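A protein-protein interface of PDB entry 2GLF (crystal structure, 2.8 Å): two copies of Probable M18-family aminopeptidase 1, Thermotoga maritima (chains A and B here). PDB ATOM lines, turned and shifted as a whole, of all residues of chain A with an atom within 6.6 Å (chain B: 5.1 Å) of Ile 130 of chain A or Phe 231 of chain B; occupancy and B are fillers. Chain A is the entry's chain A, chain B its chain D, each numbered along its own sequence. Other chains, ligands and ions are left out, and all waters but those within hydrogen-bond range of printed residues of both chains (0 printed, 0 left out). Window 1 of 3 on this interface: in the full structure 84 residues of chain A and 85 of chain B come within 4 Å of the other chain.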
ATOM      1  N   TYR A 125      10.451  15.529 -36.258  1.00  0.00           N
ATOM      2  CA  TYR A 125      10.031  16.094 -34.988  1.00  0.00           C
ATOM      3  C   TYR A 125      11.117  15.840 -33.945  1.00  0.00           C
ATOM      4  O   TYR A 125      11.106  16.436 -32.870  1.00  0.00           O
ATOM      5  CB  TYR A 125       8.682  15.523 -34.527  1.00  0.00           C
ATOM      6  CG  TYR A 125       8.602  14.022 -34.418  1.00  0.00           C
ATOM      7  CD1 TYR A 125       8.027  13.265 -35.433  1.00  0.00           C
ATOM      8  CD2 TYR A 125       9.077  13.358 -33.286  1.00  0.00           C
ATOM      9  CE1 TYR A 125       7.921  11.877 -35.324  1.00  0.00           C
ATOM     10  CE2 TYR A 125       8.978  11.973 -33.168  1.00  0.00           C
ATOM     11  CZ  TYR A 125       8.396  11.238 -34.188  1.00  0.00           C
ATOM     12  OH  TYR A 125       8.266   9.874 -34.068  1.00  0.00           O
ATOM     13  N   HIS A 126      12.062  14.960 -34.275  1.00  0.00           N
ATOM     14  CA  HIS A 126      13.173  14.647 -33.377  1.00  0.00           C
ATOM     15  C   HIS A 126      14.097  15.855 -33.223  1.00  0.00           C
ATOM     16  O   HIS A 126      14.643  16.098 -32.146  1.00  0.00           O
ATOM     17  CB  HIS A 126      14.042  13.509 -33.927  1.00  0.00           C
ATOM     18  CG  HIS A 126      13.448  12.144 -33.796  1.00  0.00           C
ATOM     19  ND1 HIS A 126      12.795  11.716 -32.661  1.00  0.00           N
ATOM     20  CD2 HIS A 126      13.476  11.081 -34.637  1.00  0.00           C
ATOM     21  CE1 HIS A 126      12.445  10.449 -32.809  1.00  0.00           C
ATOM     22  NE2 HIS A 126      12.846  10.041 -34.000  1.00  0.00           N
ATOM     23  N   TRP A 127      14.258  16.600 -34.314  1.00  0.00           N
ATOM     24  CA  TRP A 127      15.164  17.740 -34.377  1.00  0.00           C
ATOM     25  C   TRP A 127      14.694  19.074 -33.816  1.00  0.00           C
ATOM     26  O   TRP A 127      15.374  20.089 -33.975  1.00  0.00           O
ATOM     27  CB  TRP A 127      15.634  17.912 -35.828  1.00  0.00           C
ATOM     28  CG  TRP A 127      16.260  16.656 -36.346  1.00  0.00           C
ATOM     29  CD1 TRP A 127      15.617  15.478 -36.652  1.00  0.00           C
ATOM     30  CD2 TRP A 127      17.661  16.384 -36.466  1.00  0.00           C
ATOM     31  NE1 TRP A 127      16.534  14.495 -36.938  1.00  0.00           N
ATOM     32  CE2 TRP A 127      17.796  15.026 -36.832  1.00  0.00           C
ATOM     33  CE3 TRP A 127      18.817  17.154 -36.293  1.00  0.00           C
ATOM     34  CZ2 TRP A 127      19.045  14.426 -37.027  1.00  0.00           C
ATOM     35  CZ3 TRP A 127      20.056  16.555 -36.486  1.00  0.00           C
ATOM     36  CH2 TRP A 127      20.159  15.207 -36.849  1.00  0.00           C
ATOM     37  N   LEU A 128      13.549  19.083 -33.147  1.00  0.00           N
ATOM     38  CA  LEU A 128      13.051  20.321 -32.561  1.00  0.00           C
ATOM     39  C   LEU A 128      13.383  20.388 -31.065  1.00  0.00           C
ATOM     40  O   LEU A 128      13.286  19.383 -30.351  1.00  0.00           O
ATOM     41  CB  LEU A 128      11.545  20.430 -32.789  1.00  0.00           C
ATOM     42  CG  LEU A 128      11.164  20.573 -34.268  1.00  0.00           C
ATOM     43  CD1 LEU A 128       9.685  20.327 -34.452  1.00  0.00           C
ATOM     44  CD2 LEU A 128      11.548  21.960 -34.765  1.00  0.00           C
ATOM     45  N   SER A 129      13.786  21.577 -30.610  1.00  0.00           N
ATOM     46  CA  SER A 129      14.159  21.826 -29.213  1.00  0.00           C
ATOM     47  C   SER A 129      15.181  20.816 -28.697  1.00  0.00           C
ATOM     48  O   SER A 129      14.967  20.133 -27.691  1.00  0.00           O
ATOM     49  CB  SER A 129      12.917  21.828 -28.312  1.00  0.00           C
ATOM     50  OG  SER A 129      12.086  22.946 -28.589  1.00  0.00           O
ATOM     51  N   ILE A 130      16.304  20.751 -29.400  1.00  0.00           N
ATOM     52  CA  ILE A 130      17.392  19.846 -29.073  1.00  0.00           C
ATOM     53  C   ILE A 130      18.689  20.564 -29.436  1.00  0.00           C
ATOM     54  O   ILE A 130      18.786  21.162 -30.506  1.00  0.00           O
ATOM     55  CB  ILE A 130      17.206  18.519 -29.871  1.00  0.00           C
ATOM     56  CG1 ILE A 130      16.516  17.497 -28.969  1.00  0.00           C
ATOM     57  CG2 ILE A 130      18.519  17.994 -30.421  1.00  0.00           C
ATOM     58  CD1 ILE A 130      16.051  16.239 -29.693  1.00  0.00           C
ATOM     59  N   PRO A 131      19.692  20.551 -28.536  1.00  0.00           N
ATOM     60  CA  PRO A 131      20.959  21.229 -28.842  1.00  0.00           C
ATOM     61  C   PRO A 131      21.652  20.638 -30.070  1.00  0.00           C
ATOM     62  O   PRO A 131      21.766  19.419 -30.201  1.00  0.00           O
ATOM     63  CB  PRO A 131      21.775  21.051 -27.554  1.00  0.00           C
ATOM     64  CG  PRO A 131      21.254  19.778 -26.992  1.00  0.00           C
ATOM     65  CD  PRO A 131      19.757  19.895 -27.218  1.00  0.00           C
ATOM     66  N   LEU A 132      22.104  21.510 -30.969  1.00  0.00           N
ATOM     67  CA  LEU A 132      22.776  21.074 -32.188  1.00  0.00           C
ATOM     68  C   LEU A 132      24.202  21.595 -32.298  1.00  0.00           C
ATOM     69  O   LEU A 132      24.562  22.588 -31.678  1.00  0.00           O
ATOM     70  CB  LEU A 132      22.015  21.546 -33.442  1.00  0.00           C
ATOM     71  CG  LEU A 132      20.595  21.141 -33.852  1.00  0.00           C
ATOM     72  CD1 LEU A 132      20.305  19.697 -33.467  1.00  0.00           C
ATOM     73  CD2 LEU A 132      19.620  22.082 -33.209  1.00  0.00           C
ATOM     74  N   VAL A 158      25.969  26.267 -28.842  1.00  0.00           N
ATOM     75  CA  VAL A 158      25.306  25.231 -29.614  1.00  0.00           C
ATOM     76  C   VAL A 158      24.161  25.934 -30.331  1.00  0.00           C
ATOM     77  O   VAL A 158      23.965  27.139 -30.160  1.00  0.00           O
ATOM     78  CB  VAL A 158      24.730  24.109 -28.715  1.00  0.00           C
ATOM     79  CG1 VAL A 158      25.842  23.462 -27.914  1.00  0.00           C
ATOM     80  CG2 VAL A 158      23.654  24.667 -27.808  1.00  0.00           C
ATOM     81  N   PHE A 159      23.405  25.202 -31.137  1.00  0.00           N
ATOM     82  CA  PHE A 159      22.286  25.816 -31.832  1.00  0.00           C
ATOM     83  C   PHE A 159      20.991  25.063 -31.559  1.00  0.00           C
ATOM     84  O   PHE A 159      20.996  24.043 -30.874  1.00  0.00           O
ATOM     85  CB  PHE A 159      22.579  25.877 -33.327  1.00  0.00           C
ATOM     86  CG  PHE A 159      23.864  26.562 -33.641  1.00  0.00           C
ATOM     87  CD1 PHE A 159      25.074  25.891 -33.503  1.00  0.00           C
ATOM     88  CD2 PHE A 159      23.878  27.905 -34.005  1.00  0.00           C
ATOM     89  CE1 PHE A 159      26.276  26.544 -33.718  1.00  0.00           C
ATOM     90  CE2 PHE A 159      25.084  28.572 -34.222  1.00  0.00           C
ATOM     91  CZ  PHE A 159      26.281  27.891 -34.078  1.00  0.00           C
ATOM     92  N   THR A 160      19.881  25.577 -32.076  1.00  0.00           N
ATOM     93  CA  THR A 160      18.597  24.927 -31.868  1.00  0.00           C
ATOM     94  C   THR A 160      17.569  25.349 -32.888  1.00  0.00           C
ATOM     95  O   THR A 160      17.721  26.357 -33.585  1.00  0.00           O
ATOM     96  CB  THR A 160      17.969  25.276 -30.511  1.00  0.00           C
ATOM     97  OG1 THR A 160      18.995  25.594 -29.570  1.00  0.00           O
ATOM     98  CG2 THR A 160      17.156  24.106 -29.991  1.00  0.00           C
ATOM     99  N   ILE A 161      16.514  24.548 -32.952  1.00  0.00           N
ATOM    100  CA  ILE A 161      15.372  24.808 -33.796  1.00  0.00           C
ATOM    101  C   ILE A 161      14.293  24.661 -32.735  1.00  0.00           C
ATOM    102  O   ILE A 161      13.808  23.564 -32.485  1.00  0.00           O
ATOM    103  CB  ILE A 161      15.206  23.736 -34.888  1.00  0.00           C
ATOM    104  CG1 ILE A 161      16.491  23.630 -35.716  1.00  0.00           C
ATOM    105  CG2 ILE A 161      14.036  24.094 -35.792  1.00  0.00           C
ATOM    106  CD1 ILE A 161      16.484  22.500 -36.725  1.00  0.00           C
ATOM    107  N   PRO A 162      13.944  25.769 -32.060  1.00  0.00           N
ATOM    108  CA  PRO A 162      12.923  25.789 -31.002  1.00  0.00           C
ATOM    109  C   PRO A 162      11.523  25.422 -31.485  1.00  0.00           C
ATOM    110  O   PRO A 162      10.976  26.080 -32.363  1.00  0.00           O
ATOM    111  CB  PRO A 162      12.993  27.224 -30.485  1.00  0.00           C
ATOM    112  CG  PRO A 162      13.380  28.000 -31.729  1.00  0.00           C
ATOM    113  CD  PRO A 162      14.449  27.128 -32.333  1.00  0.00           C
ATOM    114  N   PRO A 229      23.277  16.510 -33.692  1.00  0.00           N
ATOM    115  CA  PRO A 229      22.973  16.610 -32.258  1.00  0.00           C
ATOM    116  C   PRO A 229      24.204  16.751 -31.355  1.00  0.00           C
ATOM    117  O   PRO A 229      25.227  16.102 -31.567  1.00  0.00           O
ATOM    118  CB  PRO A 229      22.174  15.338 -31.979  1.00  0.00           C
ATOM    119  CG  PRO A 229      22.713  14.382 -32.968  1.00  0.00           C
ATOM    120  CD  PRO A 229      22.829  15.216 -34.228  1.00  0.00           C
ATOM    121  N   ALA A 230      24.088  17.615 -30.349  1.00  0.00           N
ATOM    122  CA  ALA A 230      25.176  17.874 -29.421  1.00  0.00           C
ATOM    123  C   ALA A 230      25.268  16.807 -28.330  1.00  0.00           C
ATOM    124  O   ALA A 230      25.971  16.988 -27.335  1.00  0.00           O
ATOM    125  CB  ALA A 230      24.998  19.248 -28.803  1.00  0.00           C
ATOM    126  N   PHE A 231      24.566  15.693 -28.522  1.00  0.00           N
ATOM    127  CA  PHE A 231      24.587  14.600 -27.549  1.00  0.00           C
ATOM    128  C   PHE A 231      25.868  13.792 -27.733  1.00  0.00           C
ATOM    129  O   PHE A 231      26.228  13.457 -28.861  1.00  0.00           O
ATOM    130  CB  PHE A 231      23.411  13.651 -27.780  1.00  0.00           C
ATOM    131  CG  PHE A 231      22.085  14.335 -27.936  1.00  0.00           C
ATOM    132  CD1 PHE A 231      20.994  13.631 -28.434  1.00  0.00           C
ATOM    133  CD2 PHE A 231      21.915  15.665 -27.579  1.00  0.00           C
ATOM    134  CE1 PHE A 231      19.756  14.237 -28.571  1.00  0.00           C
ATOM    135  CE2 PHE A 231      20.681  16.282 -27.714  1.00  0.00           C
ATOM    136  CZ  PHE A 231      19.598  15.566 -28.210  1.00  0.00           C
ATOM    137  N   PRO A 427      18.142  11.064 -33.026  1.00  0.00           N
ATOM    138  CA  PRO A 427      19.365  11.776 -32.641  1.00  0.00           C
ATOM    139  C   PRO A 427      20.137  11.056 -31.532  1.00  0.00           C
ATOM    140  O   PRO A 427      21.218  11.492 -31.139  1.00  0.00           O
ATOM    141  CB  PRO A 427      18.841  13.134 -32.178  1.00  0.00           C
ATOM    142  CG  PRO A 427      17.602  13.310 -32.997  1.00  0.00           C
ATOM    143  CD  PRO A 427      16.970  11.943 -32.898  1.00  0.00           C
ATOM    144  N   LYS B  31      17.263  20.943 -11.302  1.00  0.00           N
ATOM    145  CA  LYS B  31      16.554  20.163 -12.308  1.00  0.00           C
ATOM    146  C   LYS B  31      15.137  19.826 -11.851  1.00  0.00           C
ATOM    147  O   LYS B  31      14.229  19.683 -12.669  1.00  0.00           O
ATOM    148  CB  LYS B  31      17.331  18.882 -12.638  1.00  0.00           C
ATOM    149  CG  LYS B  31      18.588  19.113 -13.467  1.00  0.00           C
ATOM    150  CD  LYS B  31      18.245  19.820 -14.774  1.00  0.00           C
ATOM    151  CE  LYS B  31      19.454  19.958 -15.696  1.00  0.00           C
ATOM    152  NZ  LYS B  31      19.929  18.645 -16.222  1.00  0.00           N
ATOM    153  N   ILE B 130      16.143  10.803 -26.565  1.00  0.00           N
ATOM    154  CA  ILE B 130      16.980  11.867 -26.044  1.00  0.00           C
ATOM    155  C   ILE B 130      17.526  11.303 -24.741  1.00  0.00           C
ATOM    156  O   ILE B 130      16.870  10.479 -24.093  1.00  0.00           O
ATOM    157  CB  ILE B 130      16.186  13.167 -25.756  1.00  0.00           C
ATOM    158  CG1 ILE B 130      15.393  13.044 -24.461  1.00  0.00           C
ATOM    159  CG2 ILE B 130      15.224  13.448 -26.894  1.00  0.00           C
ATOM    160  CD1 ILE B 130      14.661  14.312 -24.102  1.00  0.00           C
ATOM    161  N   PRO B 131      18.747  11.702 -24.361  1.00  0.00           N
ATOM    162  CA  PRO B 131      19.373  11.224 -23.121  1.00  0.00           C
ATOM    163  C   PRO B 131      18.732  11.816 -21.860  1.00  0.00           C
ATOM    164  O   PRO B 131      18.801  13.020 -21.616  1.00  0.00           O
ATOM    165  CB  PRO B 131      20.834  11.645 -23.289  1.00  0.00           C
ATOM    166  CG  PRO B 131      20.729  12.890 -24.122  1.00  0.00           C
ATOM    167  CD  PRO B 131      19.689  12.516 -25.151  1.00  0.00           C
ATOM    168  N   PRO B 229      15.630  15.913 -18.814  1.00  0.00           N
ATOM    169  CA  PRO B 229      16.628  15.961 -19.886  1.00  0.00           C
ATOM    170  C   PRO B 229      18.053  16.083 -19.358  1.00  0.00           C
ATOM    171  O   PRO B 229      18.331  16.890 -18.470  1.00  0.00           O
ATOM    172  CB  PRO B 229      16.206  17.185 -20.688  1.00  0.00           C
ATOM    173  CG  PRO B 229      14.699  17.209 -20.480  1.00  0.00           C
ATOM    174  CD  PRO B 229      14.595  16.945 -19.012  1.00  0.00           C
ATOM    175  N   ALA B 230      18.959  15.281 -19.910  1.00  0.00           N
ATOM    176  CA  ALA B 230      20.356  15.312 -19.496  1.00  0.00           C
ATOM    177  C   ALA B 230      21.105  16.494 -20.118  1.00  0.00           C
ATOM    178  O   ALA B 230      22.280  16.704 -19.832  1.00  0.00           O
ATOM    179  CB  ALA B 230      21.031  14.009 -19.871  1.00  0.00           C
ATOM    180  N   PHE B 231      20.433  17.262 -20.969  1.00  0.00           N
ATOM    181  CA  PHE B 231      21.061  18.419 -21.603  1.00  0.00           C
ATOM    182  C   PHE B 231      21.495  19.371 -20.503  1.00  0.00           C
ATOM    183  O   PHE B 231      20.724  19.646 -19.578  1.00  0.00           O
ATOM    184  CB  PHE B 231      20.071  19.185 -22.490  1.00  0.00           C
ATOM    185  CG  PHE B 231      19.374  18.346 -23.517  1.00  0.00           C
ATOM    186  CD1 PHE B 231      18.150  18.758 -24.036  1.00  0.00           C
ATOM    187  CD2 PHE B 231      19.930  17.159 -23.976  1.00  0.00           C
ATOM    188  CE1 PHE B 231      17.487  18.002 -24.998  1.00  0.00           C
ATOM    189  CE2 PHE B 231      19.275  16.393 -24.939  1.00  0.00           C
ATOM    190  CZ  PHE B 231      18.051  16.817 -25.451  1.00  0.00           C
ATOM    191  N   SER B 232      22.720  19.877 -20.608  1.00  0.00           N
ATOM    192  CA  SER B 232      23.233  20.843 -19.645  1.00  0.00           C
ATOM    193  C   SER B 232      23.071  22.230 -20.273  1.00  0.00           C
ATOM    194  O   SER B 232      23.080  22.373 -21.502  1.00  0.00           O
ATOM    195  CB  SER B 232      24.708  20.576 -19.348  1.00  0.00           C
ATOM    196  OG  SER B 232      24.867  19.390 -18.591  1.00  0.00           O
ATOM    197  N   PRO B 233      22.885  23.266 -19.445  1.00  0.00           N
ATOM    198  CA  PRO B 233      22.732  24.610 -20.000  1.00  0.00           C
ATOM    199  C   PRO B 233      23.908  24.944 -20.911  1.00  0.00           C
ATOM    200  O   PRO B 233      25.053  24.609 -20.604  1.00  0.00           O
ATOM    201  CB  PRO B 233      22.692  25.481 -18.756  1.00  0.00           C
ATOM    202  CG  PRO B 233      21.965  24.605 -17.789  1.00  0.00           C
ATOM    203  CD  PRO B 233      22.619  23.260 -17.996  1.00  0.00           C
ATOM    204  N   PRO B 427      12.337  20.118 -23.789  1.00  0.00           N
ATOM    205  CA  PRO B 427      13.516  19.752 -22.999  1.00  0.00           C
ATOM    206  C   PRO B 427      14.652  20.772 -23.072  1.00  0.00           C
ATOM    207  O   PRO B 427      15.572  20.733 -22.258  1.00  0.00           O
ATOM    208  CB  PRO B 427      13.921  18.404 -23.594  1.00  0.00           C
ATOM    209  CG  PRO B 427      12.620  17.837 -24.057  1.00  0.00           C
ATOM    210  CD  PRO B 427      11.972  19.030 -24.713  1.00  0.00           C
ATOM    211  N   PHE B 428      14.579  21.685 -24.036  1.00  0.00           N
ATOM    212  CA  PHE B 428      15.626  22.688 -24.220  1.00  0.00           C
ATOM    213  C   PHE B 428      15.009  24.040 -24.553  1.00  0.00           C
ATOM    214  O   PHE B 428      14.972  24.444 -25.710  1.00  0.00           O
ATOM    215  CB  PHE B 428      16.554  22.247 -25.360  1.00  0.00           C
ATOM    216  CG  PHE B 428      17.933  22.836 -25.293  1.00  0.00           C
ATOM    217  CD1 PHE B 428      18.761  22.584 -24.199  1.00  0.00           C
ATOM    218  CD2 PHE B 428      18.414  23.638 -26.324  1.00  0.00           C
ATOM    219  CE1 PHE B 428      20.049  23.124 -24.129  1.00  0.00           C
ATOM    220  CE2 PHE B 428      19.703  24.183 -26.264  1.00  0.00           C
ATOM    221  CZ  PHE B 428      20.519  23.924 -25.159  1.00  0.00           C
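Ile 130 of chain A touches Phe 231 of chain B, but with the chains exchanged Phe 231 of chain A does not touch Ile 130 of chain B (4.4 Å).
Pro 131 of chain A touches Phe 231 of chain B, and with the chains exchanged Phe 231 of chain A touches Pro 131 of chain B.
Phe 231 of chain B touches its own counterpart, Phe 231 of chain A.
6 positions are printed for both chains.
Of the 7 pairs that touch across the chains among the printed residues, 3 have their exchanged pair printed and touching as well.
Ser 129 of chain A touches Phe 428 of chain B (O to CB, 3.5 Å).
Ile 130 of chain A touches Phe 231 of chain B (CG1 to CZ, 3.9 Å).
Pro 131 of chain A touches Phe 231 of chain B (CD to CE1, 3.7 Å).
Phe 428 of chain B touches Pro 131 of chain A.
Thr 160 of chain A touches Phe 428 of chain B.
CD of Pro 131 of chain B touches CD1 of Phe 231 of chain A (3.7 Å).
CE2 of Phe 231 of chain A touches CE2 of Phe 231 of chain B, 3.1 Å away.
Trp 127 of chain A touches none of the printed residues of chain B.
Leu 128 of chain A touches none of the printed residues of chain B.
Ile 130 of chain A touches just one residue of chain B: Phe 231.
Of the printed residues of chain B, Pro 131 of chain A touches Phe 231 and Phe 428.
Of the printed residues of chain B, Phe 231 of chain A touches Pro 131 and Phe 231.
The nearest printed residue of chain B that does not touch Thr 160 of chain A is Phe 231 of chain B (7.9 Å).
Of the 10 printed residues of chain B, 3 touch a printed residue of chain A.
Of the 17 printed residues of chain A, 5 touch a printed residue of chain B.
Among the printed residues, no Asp or Glu carboxylate lies within 4 Å of a Lys or Arg side-chain nitrogen of the other chain.
The backbone carbonyl oxygen of Pro 131 of chain B is in hydrogen-bond range of the backbone NH of Ala 230 of chain B (2.8 Å).
The backbone carbonyl oxygen of Pro 131 of chain A is in hydrogen-bond range of the backbone NH of Ala 230 of chain A (2.9 Å).
O of Ile 161 of chain A lies within hydrogen-bond range of N of Ser 129 of chain A (2.7 Å).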
